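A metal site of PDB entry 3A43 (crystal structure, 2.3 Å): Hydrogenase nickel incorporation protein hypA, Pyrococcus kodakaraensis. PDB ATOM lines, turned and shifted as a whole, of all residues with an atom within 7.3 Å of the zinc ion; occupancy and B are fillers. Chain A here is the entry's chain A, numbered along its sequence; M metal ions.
Four residues have an atom within 4 Å of the zinc ion: Cys 73, Cys 76, Cys 110 and Cys 113. The nearest printed residue that does not touch the zinc ion is Tyr 78 (4.5 Å).
SG of Cys 76 lies close to N of Tyr 78 (3.6 Å). The backbone NH of Cys 73 lies within hydrogen-bond range of the backbone carbonyl oxygen of Tyr 78 (2.8 Å). SG of Cys 73 sits close to N of Asn 75, at 3.4 Å.
The zinc ion is bound by SG of Cys 113, SG of Cys 76, SG of Cys 110 and SG of Cys 73. The zinc ion has four donor atoms within binding distance.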
ATOM      1  N   LYS A  72     -20.084 -19.551 -10.621  1.00  0.00           N
ATOM      2  CA  LYS A  72     -19.495 -20.880 -10.665  1.00  0.00           C
ATOM      3  C   LYS A  72     -18.608 -21.083  -9.438  1.00  0.00           C
ATOM      4  O   LYS A  72     -17.548 -20.475  -9.318  1.00  0.00           O
ATOM      5  CB  LYS A  72     -18.650 -21.071 -11.927  1.00  0.00           C
ATOM      6  CG  LYS A  72     -18.046 -22.462 -12.036  1.00  0.00           C
ATOM      7  CD  LYS A  72     -17.214 -22.633 -13.299  1.00  0.00           C
ATOM      8  CE  LYS A  72     -16.682 -24.055 -13.416  1.00  0.00           C
ATOM      9  NZ  LYS A  72     -15.851 -24.244 -14.644  1.00  0.00           N
ATOM     10  N   CYS A  73     -19.068 -21.949  -8.540  1.00  0.00           N
ATOM     11  CA  CYS A  73     -18.344 -22.264  -7.310  1.00  0.00           C
ATOM     12  C   CYS A  73     -17.016 -22.937  -7.629  1.00  0.00           C
ATOM     13  O   CYS A  73     -16.986 -24.020  -8.212  1.00  0.00           O
ATOM     14  CB  CYS A  73     -19.184 -23.189  -6.448  1.00  0.00           C
ATOM     15  SG  CYS A  73     -18.371 -23.794  -4.935  1.00  0.00           S
ATOM     16  N   ARG A  74     -15.907 -22.302  -7.257  1.00  0.00           N
ATOM     17  CA  ARG A  74     -14.592 -22.870  -7.545  1.00  0.00           C
ATOM     18  C   ARG A  74     -14.192 -23.932  -6.518  1.00  0.00           C
ATOM     19  O   ARG A  74     -13.003 -24.231  -6.350  1.00  0.00           O
ATOM     20  CB  ARG A  74     -13.541 -21.757  -7.629  1.00  0.00           C
ATOM     21  CG  ARG A  74     -13.476 -20.850  -6.412  1.00  0.00           C
ATOM     22  CD  ARG A  74     -12.544 -19.652  -6.627  1.00  0.00           C
ATOM     23  NE  ARG A  74     -12.994 -18.760  -7.686  1.00  0.00           N
ATOM     24  CZ  ARG A  74     -12.427 -17.595  -7.977  1.00  0.00           C
ATOM     25  NH1 ARG A  74     -11.387 -17.171  -7.279  1.00  0.00           N
ATOM     26  NH2 ARG A  74     -12.895 -16.840  -8.973  1.00  0.00           N
ATOM     27  N   ASN A  75     -15.195 -24.518  -5.861  1.00  0.00           N
ATOM     28  CA  ASN A  75     -14.973 -25.568  -4.859  1.00  0.00           C
ATOM     29  C   ASN A  75     -15.654 -26.856  -5.285  1.00  0.00           C
ATOM     30  O   ASN A  75     -15.296 -27.930  -4.806  1.00  0.00           O
ATOM     31  CB  ASN A  75     -15.497 -25.133  -3.492  1.00  0.00           C
ATOM     32  CG  ASN A  75     -14.456 -24.388  -2.686  1.00  0.00           C
ATOM     33  OD1 ASN A  75     -13.844 -23.438  -3.164  1.00  0.00           O
ATOM     34  ND2 ASN A  75     -14.266 -24.804  -1.441  1.00  0.00           N
ATOM     35  N   CYS A  76     -16.636 -26.759  -6.166  1.00  0.00           N
ATOM     36  CA  CYS A  76     -17.335 -27.932  -6.670  1.00  0.00           C
ATOM     37  C   CYS A  76     -17.722 -27.712  -8.125  1.00  0.00           C
ATOM     38  O   CYS A  76     -18.448 -28.515  -8.723  1.00  0.00           O
ATOM     39  CB  CYS A  76     -18.583 -28.226  -5.830  1.00  0.00           C
ATOM     40  SG  CYS A  76     -19.977 -27.090  -6.098  1.00  0.00           S
ATOM     41  N   ASN A  77     -17.213 -26.614  -8.678  1.00  0.00           N
ATOM     42  CA  ASN A  77     -17.447 -26.235 -10.067  1.00  0.00           C
ATOM     43  C   ASN A  77     -18.903 -26.173 -10.481  1.00  0.00           C
ATOM     44  O   ASN A  77     -19.233 -26.282 -11.662  1.00  0.00           O
ATOM     45  CB  ASN A  77     -16.687 -27.195 -10.983  1.00  0.00           C
ATOM     46  CG  ASN A  77     -15.203 -27.193 -10.693  1.00  0.00           C
ATOM     47  OD1 ASN A  77     -14.499 -26.237 -10.995  1.00  0.00           O
ATOM     48  ND2 ASN A  77     -14.716 -28.279 -10.090  1.00  0.00           N
ATOM     49  N   TYR A  78     -19.788 -26.001  -9.500  1.00  0.00           N
ATOM     50  CA  TYR A  78     -21.218 -25.914  -9.776  1.00  0.00           C
ATOM     51  C   TYR A  78     -21.608 -24.509 -10.224  1.00  0.00           C
ATOM     52  O   TYR A  78     -21.067 -23.505  -9.734  1.00  0.00           O
ATOM     53  CB  TYR A  78     -22.004 -26.324  -8.515  1.00  0.00           C
ATOM     54  CG  TYR A  78     -23.500 -26.318  -8.712  1.00  0.00           C
ATOM     55  CD1 TYR A  78     -24.088 -26.892  -9.838  1.00  0.00           C
ATOM     56  CD2 TYR A  78     -24.343 -25.728  -7.752  1.00  0.00           C
ATOM     57  CE1 TYR A  78     -25.469 -26.884 -10.018  1.00  0.00           C
ATOM     58  CE2 TYR A  78     -25.723 -25.720  -7.931  1.00  0.00           C
ATOM     59  CZ  TYR A  78     -26.280 -26.298  -9.059  1.00  0.00           C
ATOM     60  OH  TYR A  78     -27.652 -26.275  -9.230  1.00  0.00           O
ATOM     61  N   GLU A  79     -22.539 -24.443 -11.174  1.00  0.00           N
ATOM     62  CA  GLU A  79     -23.021 -23.175 -11.718  1.00  0.00           C
ATOM     63  C   GLU A  79     -24.488 -22.916 -11.425  1.00  0.00           C
ATOM     64  O   GLU A  79     -25.349 -23.765 -11.681  1.00  0.00           O
ATOM     65  CB  GLU A  79     -22.839 -23.145 -13.244  1.00  0.00           C
ATOM     66  CG  GLU A  79     -21.478 -22.703 -13.723  1.00  0.00           C
ATOM     67  CD  GLU A  79     -21.494 -22.346 -15.204  1.00  0.00           C
ATOM     68  OE1 GLU A  79     -20.440 -21.918 -15.737  1.00  0.00           O
ATOM     69  OE2 GLU A  79     -22.561 -22.491 -15.830  1.00  0.00           O
ATOM     70  N   TRP A  80     -24.792 -21.730 -10.891  1.00  0.00           N
ATOM     71  CA  TRP A  80     -26.169 -21.399 -10.591  1.00  0.00           C
ATOM     72  C   TRP A  80     -26.480 -19.923 -10.853  1.00  0.00           C
ATOM     73  O   TRP A  80     -25.588 -19.074 -10.843  1.00  0.00           O
ATOM     74  CB  TRP A  80     -26.491 -21.730  -9.135  1.00  0.00           C
ATOM     75  CG  TRP A  80     -25.930 -20.782  -8.111  1.00  0.00           C
ATOM     76  CD1 TRP A  80     -26.622 -19.872  -7.364  1.00  0.00           C
ATOM     77  CD2 TRP A  80     -24.566 -20.684  -7.687  1.00  0.00           C
ATOM     78  NE1 TRP A  80     -25.782 -19.222  -6.502  1.00  0.00           N
ATOM     79  CE2 TRP A  80     -24.506 -19.701  -6.679  1.00  0.00           C
ATOM     80  CE3 TRP A  80     -23.388 -21.340  -8.071  1.00  0.00           C
ATOM     81  CZ2 TRP A  80     -23.321 -19.354  -6.035  1.00  0.00           C
ATOM     82  CZ3 TRP A  80     -22.203 -20.993  -7.427  1.00  0.00           C
ATOM     83  CH2 TRP A  80     -22.179 -20.014  -6.422  1.00  0.00           C
ATOM     84  N   ALA A 109     -24.164 -17.986  -2.007  1.00  0.00           N
ATOM     85  CA  ALA A 109     -23.544 -19.137  -1.375  1.00  0.00           C
ATOM     86  C   ALA A 109     -23.957 -20.315  -2.240  1.00  0.00           C
ATOM     87  O   ALA A 109     -25.142 -20.540  -2.473  1.00  0.00           O
ATOM     88  CB  ALA A 109     -24.052 -19.321   0.047  1.00  0.00           C
ATOM     89  N   CYS A 110     -22.960 -21.054  -2.730  1.00  0.00           N
ATOM     90  CA  CYS A 110     -23.226 -22.214  -3.568  1.00  0.00           C
ATOM     91  C   CYS A 110     -24.311 -23.083  -2.957  1.00  0.00           C
ATOM     92  O   CYS A 110     -24.230 -23.462  -1.788  1.00  0.00           O
ATOM     93  CB  CYS A 110     -21.941 -23.017  -3.741  1.00  0.00           C
ATOM     94  SG  CYS A 110     -22.173 -24.558  -4.659  1.00  0.00           S
ATOM     95  N   PRO A 111     -25.348 -23.417  -3.734  1.00  0.00           N
ATOM     96  CA  PRO A 111     -26.451 -24.256  -3.232  1.00  0.00           C
ATOM     97  C   PRO A 111     -26.113 -25.740  -2.984  1.00  0.00           C
ATOM     98  O   PRO A 111     -26.294 -26.231  -1.872  1.00  0.00           O
ATOM     99  CB  PRO A 111     -27.542 -24.056  -4.289  1.00  0.00           C
ATOM    100  CG  PRO A 111     -26.759 -23.830  -5.532  1.00  0.00           C
ATOM    101  CD  PRO A 111     -25.667 -22.900  -5.079  1.00  0.00           C
ATOM    102  N   LYS A 112     -25.622 -26.437  -4.014  1.00  0.00           N
ATOM    103  CA  LYS A 112     -25.292 -27.866  -3.884  1.00  0.00           C
ATOM    104  C   LYS A 112     -24.207 -28.187  -2.855  1.00  0.00           C
ATOM    105  O   LYS A 112     -24.374 -29.105  -2.049  1.00  0.00           O
ATOM    106  CB  LYS A 112     -24.900 -28.443  -5.250  1.00  0.00           C
ATOM    107  CG  LYS A 112     -26.011 -28.391  -6.294  1.00  0.00           C
ATOM    108  CD  LYS A 112     -27.071 -29.472  -6.093  1.00  0.00           C
ATOM    109  CE  LYS A 112     -26.721 -30.715  -6.901  1.00  0.00           C
ATOM    110  NZ  LYS A 112     -27.786 -31.763  -6.807  1.00  0.00           N
ATOM    111  N   CYS A 113     -23.095 -27.454  -2.883  1.00  0.00           N
ATOM    112  CA  CYS A 113     -22.033 -27.703  -1.919  1.00  0.00           C
ATOM    113  C   CYS A 113     -22.024 -26.646  -0.830  1.00  0.00           C
ATOM    114  O   CYS A 113     -23.026 -25.975  -0.611  1.00  0.00           O
ATOM    115  CB  CYS A 113     -20.648 -27.713  -2.593  1.00  0.00           C
ATOM    116  SG  CYS A 113     -19.752 -26.119  -2.540  1.00  0.00           S
ATOM    117  N   GLY A 114     -20.865 -26.532  -0.172  1.00  0.00           N
ATOM    118  CA  GLY A 114     -20.660 -25.575   0.897  1.00  0.00           C
ATOM    119  C   GLY A 114     -21.079 -24.165   0.519  1.00  0.00           C
ATOM    120  O   GLY A 114     -22.242 -23.945   0.210  1.00  0.00           O
ATOM    121  N   SER A 115     -20.145 -23.219   0.513  1.00  0.00           N
ATOM    122  CA  SER A 115     -20.522 -21.852   0.170  1.00  0.00           C
ATOM    123  C   SER A 115     -19.366 -20.905  -0.139  1.00  0.00           C
ATOM    124  O   SER A 115     -18.224 -21.134   0.254  1.00  0.00           O
ATOM    125  CB  SER A 115     -21.339 -21.225   1.296  1.00  0.00           C
ATOM    126  OG  SER A 115     -22.349 -22.102   1.794  1.00  0.00           O
ATOM    127  N   HIS A 116     -19.693 -19.820  -0.836  1.00  0.00           N
ATOM    128  CA  HIS A 116     -18.772 -18.742  -1.169  1.00  0.00           C
ATOM    129  C   HIS A 116     -17.584 -19.075  -2.050  1.00  0.00           C
ATOM    130  O   HIS A 116     -17.496 -20.150  -2.638  1.00  0.00           O
ATOM    131  CB  HIS A 116     -18.287 -18.068   0.116  1.00  0.00           C
ATOM    132  CG  HIS A 116     -19.389 -17.395   0.860  1.00  0.00           C
ATOM    133  ND1 HIS A 116     -19.762 -16.091   0.631  1.00  0.00           N
ATOM    134  CD2 HIS A 116     -20.270 -17.893   1.770  1.00  0.00           C
ATOM    135  CE1 HIS A 116     -20.837 -15.813   1.355  1.00  0.00           C
ATOM    136  NE2 HIS A 116     -21.158 -16.879   2.056  1.00  0.00           N
HETATM  137 ZN    ZN M   1     -20.035 -25.393  -4.552  1.00  0.00          ZN
